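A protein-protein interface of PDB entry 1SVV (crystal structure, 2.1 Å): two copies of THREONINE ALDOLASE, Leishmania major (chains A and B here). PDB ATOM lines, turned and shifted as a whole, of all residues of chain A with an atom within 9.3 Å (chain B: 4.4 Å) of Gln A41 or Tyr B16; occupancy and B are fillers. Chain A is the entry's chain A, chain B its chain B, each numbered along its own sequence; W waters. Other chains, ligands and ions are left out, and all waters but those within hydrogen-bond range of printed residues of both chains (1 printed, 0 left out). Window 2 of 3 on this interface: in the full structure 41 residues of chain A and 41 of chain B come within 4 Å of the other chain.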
ATOM      1  N   ASP A  37      12.377  33.990  -6.507  1.00  0.00           N
ATOM      2  CA  ASP A  37      11.204  33.998  -5.628  1.00  0.00           C
ATOM      3  C   ASP A  37      10.420  32.697  -5.722  1.00  0.00           C
ATOM      4  O   ASP A  37       9.559  32.427  -4.883  1.00  0.00           O
ATOM      5  CB  ASP A  37      10.280  35.150  -6.033  1.00  0.00           C
ATOM      6  CG  ASP A  37       9.156  35.351  -5.072  1.00  0.00           C
ATOM      7  OD1 ASP A  37       9.442  35.789  -3.938  1.00  0.00           O
ATOM      8  OD2 ASP A  37       7.960  35.083  -5.355  1.00  0.00           O
ATOM      9  N   ASN A  38      10.690  31.914  -6.761  1.00  0.00           N
ATOM     10  CA  ASN A  38      10.003  30.657  -6.983  1.00  0.00           C
ATOM     11  C   ASN A  38      10.157  29.704  -5.787  1.00  0.00           C
ATOM     12  O   ASN A  38      11.243  29.600  -5.195  1.00  0.00           O
ATOM     13  CB  ASN A  38      10.544  29.963  -8.251  1.00  0.00           C
ATOM     14  CG  ASN A  38       9.478  29.201  -8.988  1.00  0.00           C
ATOM     15  OD1 ASN A  38       8.423  29.750  -9.254  1.00  0.00           O
ATOM     16  ND2 ASN A  38       9.733  27.925  -9.307  1.00  0.00           N
ATOM     17  N   MET A  39       9.066  29.008  -5.473  1.00  0.00           N
ATOM     18  CA  MET A  39       8.962  28.072  -4.340  1.00  0.00           C
ATOM     19  C   MET A  39       8.587  28.719  -2.987  1.00  0.00           C
ATOM     20  O   MET A  39       8.319  28.014  -2.031  1.00  0.00           O
ATOM     21  CB  MET A  39      10.208  27.172  -4.210  1.00  0.00           C
ATOM     22  CG  MET A  39      10.596  26.415  -5.516  1.00  0.00           C
ATOM     23  SD  MET A  39       9.093  25.514  -6.506  1.00  0.00           S
ATOM     24  CE  MET A  39       8.882  23.872  -5.321  1.00  0.00           C
ATOM     25  N   THR A  40       8.559  30.043  -2.906  1.00  0.00           N
ATOM     26  CA  THR A  40       7.934  30.730  -1.772  1.00  0.00           C
ATOM     27  C   THR A  40       6.387  30.678  -1.895  1.00  0.00           C
ATOM     28  O   THR A  40       5.832  30.682  -3.002  1.00  0.00           O
ATOM     29  CB  THR A  40       8.415  32.195  -1.709  1.00  0.00           C
ATOM     30  OG1 THR A  40       9.832  32.235  -1.499  1.00  0.00           O
ATOM     31  CG2 THR A  40       7.859  32.930  -0.486  1.00  0.00           C
ATOM     32  N   GLN A  41       5.709  30.641  -0.754  1.00  0.00           N
ATOM     33  CA  GLN A  41       4.255  30.577  -0.713  1.00  0.00           C
ATOM     34  C   GLN A  41       3.712  31.996  -0.609  1.00  0.00           C
ATOM     35  O   GLN A  41       4.284  32.839   0.062  1.00  0.00           O
ATOM     36  CB  GLN A  41       3.781  29.690   0.440  1.00  0.00           C
ATOM     37  CG  GLN A  41       4.113  28.182   0.250  1.00  0.00           C
ATOM     38  CD  GLN A  41       3.292  27.274   1.170  1.00  0.00           C
ATOM     39  OE1 GLN A  41       3.351  27.427   2.380  1.00  0.00           O
ATOM     40  NE2 GLN A  41       2.522  26.343   0.595  1.00  0.00           N
ATOM     41  N   HIS A  42       2.640  32.261  -1.336  1.00  0.00           N
ATOM     42  CA  HIS A  42       2.047  33.585  -1.436  1.00  0.00           C
ATOM     43  C   HIS A  42       0.550  33.420  -1.358  1.00  0.00           C
ATOM     44  O   HIS A  42       0.025  32.431  -1.848  1.00  0.00           O
ATOM     45  CB  HIS A  42       2.402  34.211  -2.788  1.00  0.00           C
ATOM     46  CG  HIS A  42       3.842  34.554  -2.920  1.00  0.00           C
ATOM     47  ND1 HIS A  42       4.457  35.422  -2.052  1.00  0.00           N
ATOM     48  CD2 HIS A  42       4.798  34.127  -3.775  1.00  0.00           C
ATOM     49  CE1 HIS A  42       5.731  35.523  -2.368  1.00  0.00           C
ATOM     50  NE2 HIS A  42       5.961  34.756  -3.419  1.00  0.00           N
ATOM     51  N   ALA A  43      -0.143  34.383  -0.757  1.00  0.00           N
ATOM     52  CA  ALA A  43      -1.600  34.460  -0.882  1.00  0.00           C
ATOM     53  C   ALA A  43      -1.972  34.951  -2.297  1.00  0.00           C
ATOM     54  O   ALA A  43      -1.191  35.647  -2.939  1.00  0.00           O
ATOM     55  CB  ALA A  43      -2.168  35.370   0.156  1.00  0.00           C
ATOM     56  N   GLY A  44      -3.152  34.561  -2.770  1.00  0.00           N
ATOM     57  CA  GLY A  44      -3.582  34.812  -4.141  1.00  0.00           C
ATOM     58  C   GLY A  44      -4.293  36.132  -4.376  1.00  0.00           C
ATOM     59  O   GLY A  44      -4.519  36.913  -3.462  1.00  0.00           O
ATOM     60  N   GLN A  47      -3.214  39.748  -2.939  1.00  0.00           N
ATOM     61  CA  GLN A  47      -3.161  40.045  -1.498  1.00  0.00           C
ATOM     62  C   GLN A  47      -1.779  39.810  -0.885  1.00  0.00           C
ATOM     63  O   GLN A  47      -1.627  39.685   0.329  1.00  0.00           O
ATOM     64  CB  GLN A  47      -4.221  39.243  -0.739  1.00  0.00           C
ATOM     65  CG  GLN A  47      -5.653  39.440  -1.246  1.00  0.00           C
ATOM     66  CD  GLN A  47      -6.168  40.864  -1.096  1.00  0.00           C
ATOM     67  OE1 GLN A  47      -5.623  41.800  -1.687  1.00  0.00           O
ATOM     68  NE2 GLN A  47      -7.253  41.023  -0.345  1.00  0.00           N
ATOM     69  N   ASP A  48      -0.759  39.813  -1.723  1.00  0.00           N
ATOM     70  CA  ASP A  48       0.577  39.367  -1.316  1.00  0.00           C
ATOM     71  C   ASP A  48       1.516  40.552  -1.080  1.00  0.00           C
ATOM     72  O   ASP A  48       1.193  41.719  -1.371  1.00  0.00           O
ATOM     73  CB  ASP A  48       1.149  38.533  -2.446  1.00  0.00           C
ATOM     74  CG  ASP A  48       1.173  39.319  -3.739  1.00  0.00           C
ATOM     75  OD1 ASP A  48       2.174  40.037  -3.948  1.00  0.00           O
ATOM     76  OD2 ASP A  48       0.203  39.365  -4.542  1.00  0.00           O
ATOM     77  N   SER A  49       2.706  40.206  -0.621  1.00  0.00           N
ATOM     78  CA  SER A  49       3.798  41.144  -0.352  1.00  0.00           C
ATOM     79  C   SER A  49       4.344  41.918  -1.564  1.00  0.00           C
ATOM     80  O   SER A  49       4.799  43.057  -1.428  1.00  0.00           O
ATOM     81  CB  SER A  49       4.979  40.365   0.256  1.00  0.00           C
ATOM     82  OG  SER A  49       5.497  41.085   1.346  1.00  0.00           O
ATOM     83  N   HIS A  50       4.376  41.275  -2.728  1.00  0.00           N
ATOM     84  CA  HIS A  50       4.915  41.926  -3.920  1.00  0.00           C
ATOM     85  C   HIS A  50       4.013  43.034  -4.422  1.00  0.00           C
ATOM     86  O   HIS A  50       4.478  44.134  -4.716  1.00  0.00           O
ATOM     87  CB  HIS A  50       5.199  40.904  -4.998  1.00  0.00           C
ATOM     88  CG  HIS A  50       6.202  39.889  -4.582  1.00  0.00           C
ATOM     89  ND1 HIS A  50       7.475  40.236  -4.174  1.00  0.00           N
ATOM     90  CD2 HIS A  50       6.116  38.544  -4.462  1.00  0.00           C
ATOM     91  CE1 HIS A  50       8.133  39.139  -3.837  1.00  0.00           C
ATOM     92  NE2 HIS A  50       7.329  38.101  -4.000  1.00  0.00           N
ATOM     93  N   TRP A 251       0.773  37.885  -7.424  1.00  0.00           N
ATOM     94  CA  TRP A 251       2.079  38.393  -7.005  1.00  0.00           C
ATOM     95  C   TRP A 251       3.072  38.472  -8.155  1.00  0.00           C
ATOM     96  O   TRP A 251       4.075  39.184  -8.072  1.00  0.00           O
ATOM     97  CB  TRP A 251       2.670  37.511  -5.882  1.00  0.00           C
ATOM     98  CG  TRP A 251       3.116  36.142  -6.274  1.00  0.00           C
ATOM     99  CD1 TRP A 251       4.369  35.770  -6.674  1.00  0.00           C
ATOM    100  CD2 TRP A 251       2.340  34.939  -6.232  1.00  0.00           C
ATOM    101  NE1 TRP A 251       4.401  34.423  -6.923  1.00  0.00           N
ATOM    102  CE2 TRP A 251       3.176  33.883  -6.653  1.00  0.00           C
ATOM    103  CE3 TRP A 251       1.021  34.641  -5.871  1.00  0.00           C
ATOM    104  CZ2 TRP A 251       2.741  32.562  -6.737  1.00  0.00           C
ATOM    105  CZ3 TRP A 251       0.582  33.322  -5.961  1.00  0.00           C
ATOM    106  CH2 TRP A 251       1.444  32.297  -6.379  1.00  0.00           C
ATOM    107  N   PRO B  15       4.528  29.732   8.965  1.00  0.00           N
ATOM    108  CA  PRO B  15       3.393  28.746   8.944  1.00  0.00           C
ATOM    109  C   PRO B  15       3.191  28.177   7.545  1.00  0.00           C
ATOM    110  O   PRO B  15       2.996  28.954   6.607  1.00  0.00           O
ATOM    111  CB  PRO B  15       2.167  29.581   9.387  1.00  0.00           C
ATOM    112  CG  PRO B  15       2.742  30.823  10.027  1.00  0.00           C
ATOM    113  CD  PRO B  15       4.071  31.079   9.342  1.00  0.00           C
ATOM    114  N   TYR B  16       3.265  26.856   7.401  1.00  0.00           N
ATOM    115  CA  TYR B  16       3.086  26.223   6.099  1.00  0.00           C
ATOM    116  C   TYR B  16       1.626  26.275   5.672  1.00  0.00           C
ATOM    117  O   TYR B  16       0.754  25.961   6.466  1.00  0.00           O
ATOM    118  CB  TYR B  16       3.543  24.774   6.115  1.00  0.00           C
ATOM    119  CG  TYR B  16       3.727  24.219   4.722  1.00  0.00           C
ATOM    120  CD1 TYR B  16       4.843  24.572   3.951  1.00  0.00           C
ATOM    121  CD2 TYR B  16       2.781  23.368   4.156  1.00  0.00           C
ATOM    122  CE1 TYR B  16       5.016  24.075   2.663  1.00  0.00           C
ATOM    123  CE2 TYR B  16       2.947  22.866   2.868  1.00  0.00           C
ATOM    124  CZ  TYR B  16       4.064  23.223   2.136  1.00  0.00           C
ATOM    125  OH  TYR B  16       4.235  22.730   0.879  1.00  0.00           O
ATOM    126  N   SER B  17       1.390  26.641   4.409  1.00  0.00           N
ATOM    127  CA  SER B  17       0.054  26.777   3.844  1.00  0.00           C
ATOM    128  C   SER B  17      -0.490  25.554   3.066  1.00  0.00           C
ATOM    129  O   SER B  17       0.146  25.005   2.161  1.00  0.00           O
ATOM    130  CB  SER B  17      -0.006  28.002   2.933  1.00  0.00           C
ATOM    131  OG  SER B  17      -1.339  28.218   2.517  1.00  0.00           O
ATOM    132  N   PHE B  18      -1.702  25.164   3.443  1.00  0.00           N
ATOM    133  CA  PHE B  18      -2.510  24.178   2.744  1.00  0.00           C
ATOM    134  C   PHE B  18      -3.790  24.872   2.270  1.00  0.00           C
ATOM    135  O   PHE B  18      -4.842  24.241   2.150  1.00  0.00           O
ATOM    136  CB  PHE B  18      -2.883  23.037   3.696  1.00  0.00           C
ATOM    137  CG  PHE B  18      -1.748  22.119   4.033  1.00  0.00           C
ATOM    138  CD1 PHE B  18      -1.196  21.283   3.063  1.00  0.00           C
ATOM    139  CD2 PHE B  18      -1.259  22.048   5.335  1.00  0.00           C
ATOM    140  CE1 PHE B  18      -0.147  20.406   3.381  1.00  0.00           C
ATOM    141  CE2 PHE B  18      -0.206  21.181   5.656  1.00  0.00           C
ATOM    142  CZ  PHE B  18       0.347  20.360   4.668  1.00  0.00           C
ATOM    143  N   SER B  23      -0.360  28.537  -4.700  1.00  0.00           N
ATOM    144  CA  SER B  23       0.424  29.373  -3.772  1.00  0.00           C
ATOM    145  C   SER B  23       1.893  29.541  -4.154  1.00  0.00           C
ATOM    146  O   SER B  23       2.588  30.410  -3.620  1.00  0.00           O
ATOM    147  CB  SER B  23       0.331  28.787  -2.363  1.00  0.00           C
ATOM    148  OG  SER B  23      -0.995  28.889  -1.903  1.00  0.00           O
ATOM    149  N   VAL B  24       2.354  28.715  -5.085  1.00  0.00           N
ATOM    150  CA  VAL B  24       3.741  28.715  -5.550  1.00  0.00           C
ATOM    151  C   VAL B  24       3.743  29.015  -7.058  1.00  0.00           C
ATOM    152  O   VAL B  24       2.812  28.636  -7.766  1.00  0.00           O
ATOM    153  CB  VAL B  24       4.404  27.331  -5.263  1.00  0.00           C
ATOM    154  CG1 VAL B  24       5.786  27.224  -5.886  1.00  0.00           C
ATOM    155  CG2 VAL B  24       4.516  27.097  -3.758  1.00  0.00           C
ATOM    156  N   ASP B 315       0.972  26.640  13.370  1.00  0.00           N
ATOM    157  CA  ASP B 315       1.916  25.938  12.498  1.00  0.00           C
ATOM    158  C   ASP B 315       1.492  25.821  11.033  1.00  0.00           C
ATOM    159  O   ASP B 315       2.340  25.633  10.147  1.00  0.00           O
ATOM    160  CB  ASP B 315       2.133  24.528  13.057  1.00  0.00           C
ATOM    161  CG  ASP B 315       2.925  24.538  14.345  1.00  0.00           C
ATOM    162  OD1 ASP B 315       4.015  25.151  14.358  1.00  0.00           O
ATOM    163  OD2 ASP B 315       2.537  23.973  15.392  1.00  0.00           O
ATOM    164  N   PHE B 316       0.192  25.931  10.771  1.00  0.00           N
ATOM    165  CA  PHE B 316      -0.349  25.677   9.439  1.00  0.00           C
ATOM    166  C   PHE B 316      -1.483  26.625   9.063  1.00  0.00           C
ATOM    167  O   PHE B 316      -2.237  27.085   9.917  1.00  0.00           O
ATOM    168  CB  PHE B 316      -0.837  24.237   9.340  1.00  0.00           C
ATOM    169  CG  PHE B 316       0.215  23.225   9.658  1.00  0.00           C
ATOM    170  CD1 PHE B 316       1.155  22.863   8.703  1.00  0.00           C
ATOM    171  CD2 PHE B 316       0.285  22.647  10.919  1.00  0.00           C
ATOM    172  CE1 PHE B 316       2.133  21.928   8.992  1.00  0.00           C
ATOM    173  CE2 PHE B 316       1.275  21.716  11.215  1.00  0.00           C
ATOM    174  CZ  PHE B 316       2.197  21.358  10.247  1.00  0.00           C
ATOM    175  N   ASP B 317      -1.606  26.902   7.770  1.00  0.00           N
ATOM    176  CA  ASP B 317      -2.688  27.731   7.265  1.00  0.00           C
ATOM    177  C   ASP B 317      -3.680  26.871   6.483  1.00  0.00           C
ATOM    178  O   ASP B 317      -3.303  26.160   5.545  1.00  0.00           O
ATOM    179  CB  ASP B 317      -2.140  28.858   6.381  1.00  0.00           C
ATOM    180  CG  ASP B 317      -2.148  30.202   7.083  1.00  0.00           C
ATOM    181  OD1 ASP B 317      -3.251  30.770   7.266  1.00  0.00           O
ATOM    182  OD2 ASP B 317      -1.112  30.767   7.487  1.00  0.00           O
ATOM    183  N   ALA B 338       3.538  21.306  -5.681  1.00  0.00           N
ATOM    184  CA  ALA B 338       4.629  21.923  -4.949  1.00  0.00           C
ATOM    185  C   ALA B 338       4.655  21.548  -3.480  1.00  0.00           C
ATOM    186  O   ALA B 338       5.577  21.928  -2.770  1.00  0.00           O
ATOM    187  CB  ALA B 338       4.521  23.423  -5.076  1.00  0.00           C
ATOM    188  N   THR B 339       3.647  20.824  -3.018  1.00  0.00           N
ATOM    189  CA  THR B 339       3.529  20.509  -1.598  1.00  0.00           C
ATOM    190  C   THR B 339       4.676  19.602  -1.161  1.00  0.00           C
ATOM    191  O   THR B 339       5.000  18.633  -1.849  1.00  0.00           O
ATOM    192  CB  THR B 339       2.163  19.855  -1.286  1.00  0.00           C
ATOM    193  OG1 THR B 339       1.108  20.813  -1.449  1.00  0.00           O
ATOM    194  CG2 THR B 339       2.057  19.439   0.177  1.00  0.00           C
ATOM    195  N   GLU B 340       5.256  19.922  -0.004  1.00  0.00           N
ATOM    196  CA  GLU B 340       6.403  19.204   0.564  1.00  0.00           C
ATOM    197  C   GLU B 340       5.915  18.053   1.431  1.00  0.00           C
ATOM    198  O   GLU B 340       5.067  18.247   2.310  1.00  0.00           O
ATOM    199  CB  GLU B 340       7.263  20.152   1.414  1.00  0.00           C
ATOM    200  CG  GLU B 340       8.216  21.045   0.623  1.00  0.00           C
ATOM    201  CD  GLU B 340       8.965  22.047   1.500  1.00  0.00           C
ATOM    202  OE1 GLU B 340       9.943  21.644   2.175  1.00  0.00           O
ATOM    203  OE2 GLU B 340       8.586  23.243   1.512  1.00  0.00           O
ATOM    204  N   GLU B 343       6.228  18.461   5.245  1.00  0.00           N
ATOM    205  CA  GLU B 343       5.178  19.261   5.859  1.00  0.00           C
ATOM    206  C   GLU B 343       3.915  18.442   6.098  1.00  0.00           C
ATOM    207  O   GLU B 343       3.184  18.686   7.059  1.00  0.00           O
ATOM    208  CB  GLU B 343       4.844  20.473   4.998  1.00  0.00           C
ATOM    209  CG  GLU B 343       5.986  21.467   4.913  1.00  0.00           C
ATOM    210  CD  GLU B 343       6.336  22.093   6.253  1.00  0.00           C
ATOM    211  OE1 GLU B 343       5.498  22.046   7.183  1.00  0.00           O
ATOM    212  OE2 GLU B 343       7.459  22.623   6.376  1.00  0.00           O
HETATM  213  O   HOH W   1      -2.290  31.646  -3.360  1.00  0.00           O
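The side-chain amide oxygen (OE1) of Gln A41 is in hydrogen-bond range of the backbone NH (N) of Ser B17 (2.9 Å). The backbone NH (N) of His A42 lies within hydrogen-bond range of the backbone carbonyl oxygen (O) of Ser B23 (2.9 Å). The backbone carbonyl oxygen of Thr A40 lies close to the backbone carbonyl oxygen of Ser B23.
The backbone carbonyl oxygen (O) of Asp A37 sits close to the side-chain hydroxyl (OG1) of Thr A40 (3.4 Å). The side-chain sulfur (SD) of Met A39 sits at hydrogen-bond distance from the side-chain amide nitrogen (ND2) of Asn A38 (3.8 Å). The side-chain carboxylate (OD2) of Asp A48 sits close to the backbone NH (N) of Trp A251 (3.3 Å). O of Asp B315 sits at hydrogen-bond distance from N of Tyr B16, at 3.1 Å. The backbone carbonyl oxygen of Tyr B16 is in hydrogen-bond range of the backbone NH of Asp B317 (2.9 Å). OH of Tyr B16 sits at hydrogen-bond distance from N of Glu B340 (3.1 Å).
Among the printed residues, merely in contact across the chains: Gln A41 with Ser B23, Trp A251 with Ser B23, Gln A41 with Tyr B16, Met A39 with Val B24, Trp A251 with Val B24 and Thr A40 with Val B24.
Of chain B, only Tyr B16, Ser B17 and Ser B23 come within 4 Å of Gln A41. Of chain A, only Gln A41 comes within 4 Å of Tyr B16. No residue of chain A comes within 4 Å of Pro B15. Ser B17 touches just one residue of chain A: Gln A41 (2.9 Å). Printed residues of chain A within 4 Å of Ser B23: Thr A40, Gln A41, His A42 and Trp A251. Printed residues of chain B within 4 Å of Trp A251: Ser B23 (3.5 Å) and Val B24 (3.7 Å). Of the printed residues of chain B, His A42 touches Ser B23 (2.9 Å). Ser A49 touches none of the printed residues of chain B. Asp B317 touches none of the printed residues of chain A. The nearest residue of chain A that does not touch Tyr B16 is Met A39 (7.0 Å). The nearest printed residue of chain B that does not touch Thr A40 is Ala B338 (7.7 Å).
Hydrophobic or aromatic side chains of chain B that line the printed part of chain A: Tyr B16 and Val B24. Among the printed residues, 9 pairs touch across the chains. Among the printed residues, no Asp or Glu carboxylate lies within 4 Å of a Lys or Arg side-chain nitrogen of the other chain.
No position is printed for both chains.
Water W1 lies within hydrogen-bond range of the backbone carbonyl oxygen of His A42 (2.9 Å), the backbone NH of Gly A44 (3.1 Å) and the side-chain hydroxyl of Ser B23 (3.4 Å).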
